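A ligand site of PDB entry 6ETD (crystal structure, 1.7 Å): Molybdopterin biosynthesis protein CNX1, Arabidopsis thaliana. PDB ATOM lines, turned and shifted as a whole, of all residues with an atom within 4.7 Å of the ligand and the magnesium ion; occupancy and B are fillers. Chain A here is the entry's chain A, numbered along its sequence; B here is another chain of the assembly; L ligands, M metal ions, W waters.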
ATOM      1  N   SER A 202       8.615 -21.338  24.023  1.00  0.00           N
ATOM      2  CA  SER A 202       9.202 -22.480  23.321  1.00  0.00           C
ATOM      3  C   SER A 202       8.094 -23.474  23.133  1.00  0.00           C
ATOM      4  O   SER A 202       7.119 -23.477  23.899  1.00  0.00           O
ATOM      5  CB  SER A 202      10.327 -23.113  24.144  1.00  0.00           C
ATOM      6  OG  SER A 202      11.457 -22.265  24.041  1.00  0.00           O
ATOM      7  N   THR A 203       8.230 -24.323  22.123  1.00  0.00           N
ATOM      8  CA  THR A 203       7.237 -25.352  21.855  1.00  0.00           C
ATOM      9  C   THR A 203       7.902 -26.731  21.753  1.00  0.00           C
ATOM     10  O   THR A 203       8.979 -26.853  21.160  1.00  0.00           O
ATOM     11  CB  THR A 203       6.411 -25.071  20.582  1.00  0.00           C
ATOM     12  OG1 THR A 203       7.194 -25.261  19.403  1.00  0.00           O
ATOM     13  CG2 THR A 203       5.739 -23.690  20.583  1.00  0.00           C
ATOM     14  N   GLY A 204       7.231 -27.738  22.269  1.00  0.00           N
ATOM     15  CA  GLY A 204       7.676 -29.124  22.114  1.00  0.00           C
ATOM     16  C   GLY A 204       7.396 -30.065  23.259  1.00  0.00           C
ATOM     17  O   GLY A 204       7.749 -29.777  24.400  1.00  0.00           O
ATOM     18  N   GLU A 206       9.087 -32.765  23.554  1.00  0.00           N
ATOM     19  CA  GLU A 206      10.420 -33.274  23.870  1.00  0.00           C
ATOM     20  C   GLU A 206      11.180 -32.358  24.822  1.00  0.00           C
ATOM     21  O   GLU A 206      12.186 -32.786  25.355  1.00  0.00           O
ATOM     22  CB  GLU A 206      11.263 -33.553  22.584  1.00  0.00           C
ATOM     23  CG  GLU A 206      11.933 -32.356  21.915  1.00  0.00           C
ATOM     24  CD  GLU A 206      11.032 -31.447  21.107  1.00  0.00           C
ATOM     25  OE1 GLU A 206       9.791 -31.529  21.257  1.00  0.00           O
ATOM     26  OE2 GLU A 206      11.578 -30.665  20.306  1.00  0.00           O
ATOM     27  N   LEU A 207      10.756 -31.095  24.987  1.00  0.00           N
ATOM     28  CA  LEU A 207      11.473 -30.136  25.840  1.00  0.00           C
ATOM     29  C   LEU A 207      11.277 -30.338  27.330  1.00  0.00           C
ATOM     30  O   LEU A 207      10.168 -30.654  27.790  1.00  0.00           O
ATOM     31  CB  LEU A 207      11.044 -28.687  25.512  1.00  0.00           C
ATOM     32  CG  LEU A 207      11.201 -28.222  24.064  1.00  0.00           C
ATOM     33  CD1 LEU A 207      10.758 -26.754  23.921  1.00  0.00           C
ATOM     34  CD2 LEU A 207      12.645 -28.395  23.572  1.00  0.00           C
ATOM     35  N   ILE A 220      15.162 -33.207  25.660  1.00  0.00           N
ATOM     36  CA  ILE A 220      16.281 -32.276  25.528  1.00  0.00           C
ATOM     37  C   ILE A 220      15.940 -31.068  26.374  1.00  0.00           C
ATOM     38  O   ILE A 220      14.749 -30.757  26.546  1.00  0.00           O
ATOM     39  CB  ILE A 220      16.579 -31.851  24.053  1.00  0.00           C
ATOM     40  CG1 ILE A 220      15.351 -31.122  23.404  1.00  0.00           C
ATOM     41  CG2 ILE A 220      16.984 -33.084  23.249  1.00  0.00           C
ATOM     42  CD1 ILE A 220      15.640 -30.451  22.125  1.00  0.00           C
ATOM     43  N   ARG A 221      16.967 -30.330  26.838  1.00  0.00           N
ATOM     44  CA  ARG A 221      16.709 -29.099  27.571  1.00  0.00           C
ATOM     45  C   ARG A 221      16.282 -28.002  26.595  1.00  0.00           C
ATOM     46  O   ARG A 221      16.824 -27.873  25.492  1.00  0.00           O
ATOM     47  CB  ARG A 221      17.963 -28.628  28.336  1.00  0.00           C
ATOM     48  CG  ARG A 221      18.299 -29.605  29.461  1.00  0.00           C
ATOM     49  CD  ARG A 221      19.415 -29.178  30.409  1.00  0.00           C
ATOM     50  NE  ARG A 221      19.797 -30.333  31.209  1.00  0.00           N
ATOM     51  CZ  ARG A 221      20.651 -31.295  30.837  1.00  0.00           C
ATOM     52  NH1 ARG A 221      21.291 -31.201  29.679  1.00  0.00           N
ATOM     53  NH2 ARG A 221      20.873 -32.324  31.630  1.00  0.00           N
ATOM     54  N   ASP A 222      15.316 -27.182  27.031  1.00  0.00           N
ATOM     55  CA  ASP A 222      14.867 -26.026  26.258  1.00  0.00           C
ATOM     56  C   ASP A 222      16.031 -25.005  26.243  1.00  0.00           C
ATOM     57  O   ASP A 222      16.323 -24.426  27.267  1.00  0.00           O
ATOM     58  CB  ASP A 222      13.639 -25.397  26.921  1.00  0.00           C
ATOM     59  CG  ASP A 222      13.136 -24.102  26.310  1.00  0.00           C
ATOM     60  OD1 ASP A 222      13.649 -23.703  25.257  1.00  0.00           O
ATOM     61  OD2 ASP A 222      12.214 -23.505  26.853  1.00  0.00           O
ATOM     62  N   SER A 223      16.731 -24.856  25.103  1.00  0.00           N
ATOM     63  CA  SER A 223      17.835 -23.898  25.010  1.00  0.00           C
ATOM     64  C   SER A 223      17.409 -22.616  24.257  1.00  0.00           C
ATOM     65  O   SER A 223      17.953 -21.550  24.538  1.00  0.00           O
ATOM     66  CB  SER A 223      19.055 -24.538  24.353  1.00  0.00           C
ATOM     67  OG  SER A 223      18.806 -24.883  23.003  1.00  0.00           O
ATOM     68  N   ASN A 224      16.473 -22.710  23.309  1.00  0.00           N
ATOM     69  CA  ASN A 224      16.040 -21.535  22.523  1.00  0.00           C
ATOM     70  C   ASN A 224      15.433 -20.414  23.356  1.00  0.00           C
ATOM     71  O   ASN A 224      15.673 -19.242  23.036  1.00  0.00           O
ATOM     72  CB  ASN A 224      15.022 -21.948  21.436  1.00  0.00           C
ATOM     73  CG  ASN A 224      15.573 -22.709  20.251  1.00  0.00           C
ATOM     74  OD1 ASN A 224      16.782 -22.893  20.108  1.00  0.00           O
ATOM     75  ND2 ASN A 224      14.686 -23.203  19.395  1.00  0.00           N
ATOM     76  N   ARG A 225      14.633 -20.747  24.386  1.00  0.00           N
ATOM     77  CA  ARG A 225      13.984 -19.711  25.176  1.00  0.00           C
ATOM     78  C   ARG A 225      14.990 -18.821  25.896  1.00  0.00           C
ATOM     79  O   ARG A 225      14.870 -17.597  25.769  1.00  0.00           O
ATOM     80  CB  ARG A 225      12.998 -20.307  26.181  1.00  0.00           C
ATOM     81  CG  ARG A 225      12.094 -19.275  26.896  1.00  0.00           C
ATOM     82  CD  ARG A 225      10.786 -19.962  27.306  1.00  0.00           C
ATOM     83  NE  ARG A 225      11.089 -21.255  27.953  1.00  0.00           N
ATOM     84  CZ  ARG A 225      11.298 -21.466  29.245  1.00  0.00           C
ATOM     85  NH1 ARG A 225      11.118 -20.486  30.132  1.00  0.00           N
ATOM     86  NH2 ARG A 225      11.625 -22.669  29.681  1.00  0.00           N
ATOM     87  N   ASP A 247       2.873 -29.535  22.288  1.00  0.00           N
ATOM     88  CA  ASP A 247       2.358 -29.670  20.910  1.00  0.00           C
ATOM     89  C   ASP A 247       0.875 -30.046  20.947  1.00  0.00           C
ATOM     90  O   ASP A 247       0.457 -31.133  20.558  1.00  0.00           O
ATOM     91  CB  ASP A 247       3.206 -30.688  20.098  1.00  0.00           C
ATOM     92  CG  ASP A 247       4.680 -30.289  20.068  1.00  0.00           C
ATOM     93  OD1 ASP A 247       4.973 -29.082  19.918  1.00  0.00           O
ATOM     94  OD2 ASP A 247       5.536 -31.182  20.230  1.00  0.00           O
ATOM     95  N   SER A 270       9.364 -20.492  18.992  1.00  0.00           N
ATOM     96  CA  SER A 270      10.338 -21.293  18.248  1.00  0.00           C
ATOM     97  C   SER A 270       9.783 -22.705  18.179  1.00  0.00           C
ATOM     98  O   SER A 270       9.038 -23.116  19.062  1.00  0.00           O
ATOM     99  CB  SER A 270      11.748 -21.223  18.828  1.00  0.00           C
ATOM    100  OG  SER A 270      11.941 -22.034  19.982  1.00  0.00           O
ATOM    101  N   GLY A 271      10.103 -23.419  17.104  1.00  0.00           N
ATOM    102  CA  GLY A 271       9.626 -24.770  16.896  1.00  0.00           C
ATOM    103  C   GLY A 271       8.183 -24.776  16.405  1.00  0.00           C
ATOM    104  O   GLY A 271       7.580 -23.720  16.261  1.00  0.00           O
ATOM    105  N   GLY A 272       7.643 -25.979  16.171  1.00  0.00           N
ATOM    106  CA  GLY A 272       6.267 -26.167  15.719  1.00  0.00           C
ATOM    107  C   GLY A 272       5.909 -25.484  14.414  1.00  0.00           C
ATOM    108  O   GLY A 272       4.748 -25.125  14.208  1.00  0.00           O
ATOM    109  N   VAL A 273       6.926 -25.238  13.538  1.00  0.00           N
ATOM    110  CA  VAL A 273       6.755 -24.551  12.238  1.00  0.00           C
ATOM    111  C   VAL A 273       7.307 -25.382  11.088  1.00  0.00           C
ATOM    112  O   VAL A 273       7.472 -24.829  10.022  1.00  0.00           O
ATOM    113  CB  VAL A 273       7.384 -23.107  12.214  1.00  0.00           C
ATOM    114  CG1 VAL A 273       6.457 -22.081  12.828  1.00  0.00           C
ATOM    115  CG2 VAL A 273       8.752 -23.075  12.873  1.00  0.00           C
ATOM    116  N   SER A 274       7.601 -26.696  11.280  1.00  0.00           N
ATOM    117  CA  SER A 274       8.111 -27.526  10.174  1.00  0.00           C
ATOM    118  C   SER A 274       6.917 -28.283   9.549  1.00  0.00           C
ATOM    119  O   SER A 274       5.808 -27.739   9.506  1.00  0.00           O
ATOM    120  CB  SER A 274       9.212 -28.473  10.657  1.00  0.00           C
ATOM    121  OG  SER A 274      10.214 -27.846  11.438  1.00  0.00           O
ATOM    122  N   ASP A 279       2.615 -29.529  14.378  1.00  0.00           N
ATOM    123  CA  ASP A 279       3.243 -28.193  14.217  1.00  0.00           C
ATOM    124  C   ASP A 279       2.077 -27.217  13.981  1.00  0.00           C
ATOM    125  O   ASP A 279       1.558 -27.132  12.872  1.00  0.00           O
ATOM    126  CB  ASP A 279       4.236 -28.215  13.028  1.00  0.00           C
ATOM    127  CG  ASP A 279       5.560 -28.911  13.344  1.00  0.00           C
ATOM    128  OD1 ASP A 279       5.793 -29.243  14.528  1.00  0.00           O
ATOM    129  OD2 ASP A 279       6.353 -29.115  12.425  1.00  0.00           O
ATOM    130  N   GLY A 329      12.702 -24.128  15.010  1.00  0.00           N
ATOM    131  CA  GLY A 329      13.123 -24.812  16.238  1.00  0.00           C
ATOM    132  C   GLY A 329      14.621 -25.063  16.323  1.00  0.00           C
ATOM    133  O   GLY A 329      15.202 -25.001  17.405  1.00  0.00           O
ATOM    134  N   ASN A 330      15.261 -25.416  15.187  1.00  0.00           N
ATOM    135  CA  ASN A 330      16.710 -25.670  15.192  1.00  0.00           C
ATOM    136  C   ASN A 330      17.470 -24.482  15.791  1.00  0.00           C
ATOM    137  O   ASN A 330      17.285 -23.351  15.328  1.00  0.00           O
ATOM    138  CB  ASN A 330      17.224 -25.989  13.790  1.00  0.00           C
ATOM    139  CG  ASN A 330      16.948 -27.407  13.353  1.00  0.00           C
ATOM    140  OD1 ASN A 330      17.279 -28.380  14.052  1.00  0.00           O
ATOM    141  ND2 ASN A 330      16.327 -27.564  12.218  1.00  0.00           N
ATOM    142  N   PRO A 331      18.228 -24.701  16.898  1.00  0.00           N
ATOM    143  CA  PRO A 331      18.879 -23.567  17.592  1.00  0.00           C
ATOM    144  C   PRO A 331      19.625 -22.552  16.739  1.00  0.00           C
ATOM    145  O   PRO A 331      19.489 -21.367  16.975  1.00  0.00           O
ATOM    146  CB  PRO A 331      19.828 -24.279  18.559  1.00  0.00           C
ATOM    147  CG  PRO A 331      19.073 -25.482  18.952  1.00  0.00           C
ATOM    148  CD  PRO A 331      18.451 -25.962  17.648  1.00  0.00           C
ATOM    149  N   THR B 112      10.515 -33.932  13.208  1.00  0.00           N
ATOM    150  CA  THR B 112      11.883 -33.446  13.447  1.00  0.00           C
ATOM    151  C   THR B 112      12.118 -33.402  14.947  1.00  0.00           C
ATOM    152  O   THR B 112      11.239 -32.936  15.672  1.00  0.00           O
ATOM    153  CB  THR B 112      12.091 -32.073  12.799  1.00  0.00           C
ATOM    154  OG1 THR B 112      11.741 -32.167  11.425  1.00  0.00           O
ATOM    155  CG2 THR B 112      13.540 -31.574  12.924  1.00  0.00           C
ATOM    156  N   GLY B 113      13.210 -34.004  15.399  1.00  0.00           N
ATOM    157  CA  GLY B 113      13.560 -34.085  16.803  1.00  0.00           C
ATOM    158  C   GLY B 113      12.984 -35.302  17.510  1.00  0.00           C
ATOM    159  O   GLY B 113      13.285 -35.532  18.671  1.00  0.00           O
ATOM    160  N   ARG B 155      20.292 -37.585  13.281  1.00  0.00           N
ATOM    161  CA  ARG B 155      21.347 -36.989  14.097  1.00  0.00           C
ATOM    162  C   ARG B 155      21.719 -38.088  15.097  1.00  0.00           C
ATOM    163  O   ARG B 155      20.932 -38.348  16.018  1.00  0.00           O
ATOM    164  CB  ARG B 155      20.826 -35.771  14.858  1.00  0.00           C
ATOM    165  CG  ARG B 155      20.751 -34.523  13.991  1.00  0.00           C
ATOM    166  CD  ARG B 155      19.822 -33.493  14.591  1.00  0.00           C
ATOM    167  NE  ARG B 155      20.314 -33.045  15.903  1.00  0.00           N
ATOM    168  CZ  ARG B 155      19.581 -32.826  16.985  1.00  0.00           C
ATOM    169  NH1 ARG B 155      18.262 -33.002  16.969  1.00  0.00           N
ATOM    170  NH2 ARG B 155      20.165 -32.417  18.116  1.00  0.00           N
HETATM  171  P1  LIG L   1      10.262 -28.353  15.256  1.00  0.00           P
HETATM  172  O1  LIG L   1      10.187 -29.752  14.678  1.00  0.00           O
HETATM  173  O2  LIG L   1       9.389 -28.137  16.472  1.00  0.00           O
HETATM  174  O3  LIG L   1      10.113 -27.284  14.224  1.00  0.00           O
HETATM  175  O4  LIG L   1      11.782 -28.270  15.789  1.00  0.00           O
HETATM  176  C1  LIG L   1      12.931 -28.456  14.954  1.00  0.00           C
HETATM  177  C2  LIG L   1      14.134 -28.948  15.762  1.00  0.00           C
HETATM  178  O5  LIG L   1      14.515 -27.987  16.762  1.00  0.00           O
HETATM  179  C3  LIG L   1      13.881 -30.258  16.515  1.00  0.00           C
HETATM  180  O6  LIG L   1      15.072 -31.060  16.436  1.00  0.00           O
HETATM  181  C4  LIG L   1      13.602 -29.805  17.946  1.00  0.00           C
HETATM  182  O7  LIG L   1      13.825 -30.815  18.957  1.00  0.00           O
HETATM  183  C5  LIG L   1      14.499 -28.574  18.059  1.00  0.00           C
HETATM  184  N1  LIG L   1      13.958 -27.603  19.029  1.00  0.00           N
HETATM  185  C6  LIG L   1      12.709 -27.068  19.000  1.00  0.00           C
HETATM  186  N2  LIG L   1      12.533 -26.236  20.042  1.00  0.00           N
HETATM  187  C7  LIG L   1      13.707 -26.202  20.727  1.00  0.00           C
HETATM  188  C8  LIG L   1      14.216 -25.526  21.937  1.00  0.00           C
HETATM  189  N3  LIG L   1      13.435 -24.688  22.619  1.00  0.00           N
HETATM  190  N4  LIG L   1      15.489 -25.744  22.342  1.00  0.00           N
HETATM  191  C9  LIG L   1      16.284 -26.598  21.668  1.00  0.00           C
HETATM  192  N5  LIG L   1      15.881 -27.270  20.567  1.00  0.00           N
HETATM  193  C10 LIG L   1      14.633 -27.101  20.056  1.00  0.00           C
HETATM  194 MG    MG M   1       8.672 -29.396  17.975  1.00  0.00          MG
HETATM  195  O   HOH W   1       7.189 -27.978  18.649  1.00  0.00           O
HETATM  196  O   HOH W   2      11.446 -25.411  12.915  1.00  0.00           O
HETATM  197  O   HOH W   3      10.198 -30.983  17.554  1.00  0.00           O
HETATM  198  O   HOH W   4      15.975 -32.750  19.103  1.00  0.00           O
HETATM  199  O   HOH W   5       7.240 -30.294  16.581  1.00  0.00           O
HETATM  200  O   HOH W   6      10.862 -24.265  21.077  1.00  0.00           O
HETATM  201  O   HOH W   7      16.434 -32.718  14.659  1.00  0.00           O
HETATM  202  O   HOH W   8      18.274 -28.773  20.202  1.00  0.00           O
HETATM  203  O   HOH W   9       8.172 -30.836  13.331  1.00  0.00           O
HETATM  204  O   HOH W  10      10.053 -28.672  19.401  1.00  0.00           O
HETATM  205  O   HOH W  11       8.051 -30.970  19.243  1.00  0.00           O
HETATM  206  O   HOH W  12      17.527 -29.607  16.401  1.00  0.00           O
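The backbone carbonyl oxygen of Glu 206 lies within hydrogen-bond range of the backbone NH of Ile 220. OG1 of Thr 203 lies within hydrogen-bond range of N of Gly 272 (3.3 Å). OD1 of Asp 222 sits at hydrogen-bond distance from OG of Ser 202 (2.9 Å). OD2 of Asp 222 lies within salt-bridge range of NE of Arg 225. The side-chain carboxylate of Asp 279 sits at hydrogen-bond distance from the backbone NH of Ser 274. The backbone carbonyl oxygen of Gly 329 is in hydrogen-bond range of the side-chain amide nitrogen of Asn 224, at 2.7 Å. OG of Ser 270 lies within hydrogen-bond range of ND2 of Asn 224 (3.0 Å). The backbone carbonyl oxygen of Ser 270 lies within hydrogen-bond range of the side-chain hydroxyl of Thr 203.
The backbone carbonyl oxygen (O) of Gly 329 sits close to an oxygen (O5) of the ligand (3.1 Å). The backbone carbonyl oxygen of Thr 112 of chain B sits close to an oxygen (O1) of the ligand (3.5 Å). Merely in contact with the ligand: Thr 203, Leu 207, Ile 220, Gly 271, Val 273, Pro 331, Gly 113 of chain B and Arg 155 of chain B. Hydrophobic or aromatic side chains within 4 Å of the ligand: Leu 207, Ile 220 and Pro 331. The nearest printed residue that does not touch the ligand is Ser 270 (4.03 Å).
O2 of the ligand is bound to the magnesium ion (2.1 Å). Water W10 is bound to the magnesium ion (2.1 Å). Water W11 is bound to the magnesium ion. Water W1 binds the magnesium ion (2.2 Å). The magnesium ion is bound by water W5, 2.2 Å away. Water W3 binds the magnesium ion, at 2.2 Å. The magnesium ion has six donor atoms within binding distance.
Merely in contact with the magnesium ion: Glu 206 (3.9 Å) and Gly 272 (3.999 Å). Of the 24 residues printed, 2 come within 4 Å of the magnesium ion. The nearest printed residue that does not touch the magnesium ion is Thr 203 (4.1 Å).
Water W1 lies within hydrogen-bond range of the side-chain carboxylate of Asp 247, the side-chain hydroxyl of Thr 203 and the backbone NH of Gly 272. Water W10 lies within hydrogen-bond range of the side-chain carboxylate of Glu 206 (2.7 Å) and the backbone carbonyl oxygen of Thr 203 (2.7 Å). Water W2 lies within hydrogen-bond range of an oxygen (O3) of the ligand (2.6 Å), the backbone NH (N) of Gly 329 (2.8 Å) and the side-chain hydroxyl (OG) of Ser 274 (3.1 Å). Water W6 lies within hydrogen-bond range of the side-chain hydroxyl of Ser 270 (2.7 Å), a nitrogen (N2) of the ligand (2.8 Å) and the backbone NH of Thr 203 (2.8 Å). Water W7 lies within hydrogen-bond range of O6 of the ligand and NH1 of Arg 155 of chain B. Water W4 lies within hydrogen-bond range of O7 of the ligand and NH1 of Arg 155 of chain B.
The side-chain carboxylate of Glu 206 lies within hydrogen-bond range of an oxygen (O7) of the ligand (2.6 Å). The backbone NH (N) of Gly 272 lies within hydrogen-bond range of an oxygen (O3) of the ligand, at 3.4 Å. A nitrogen (N3) of the ligand lies within hydrogen-bond range of the side-chain carboxylate (OD1) of Asp 222. An oxygen (O3) of the ligand lies within hydrogen-bond range of the side-chain hydroxyl (OG) of Ser 274 (2.8 Å). The backbone NH (N) of Asn 330 sits at hydrogen-bond distance from an oxygen (O5) of the ligand (3.1 Å). The backbone NH (N) of Ser 223 sits at hydrogen-bond distance from a nitrogen (N4) of the ligand (3.2 Å). The side-chain hydroxyl of Ser 223 lies close to a nitrogen (N4) of the ligand, 3.5 Å away. N of Asn 224 is in hydrogen-bond range of N4 of the ligand (3.3 Å). The side-chain hydroxyl (OG) of Ser 202 is in hydrogen-bond range of a nitrogen (N3) of the ligand.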
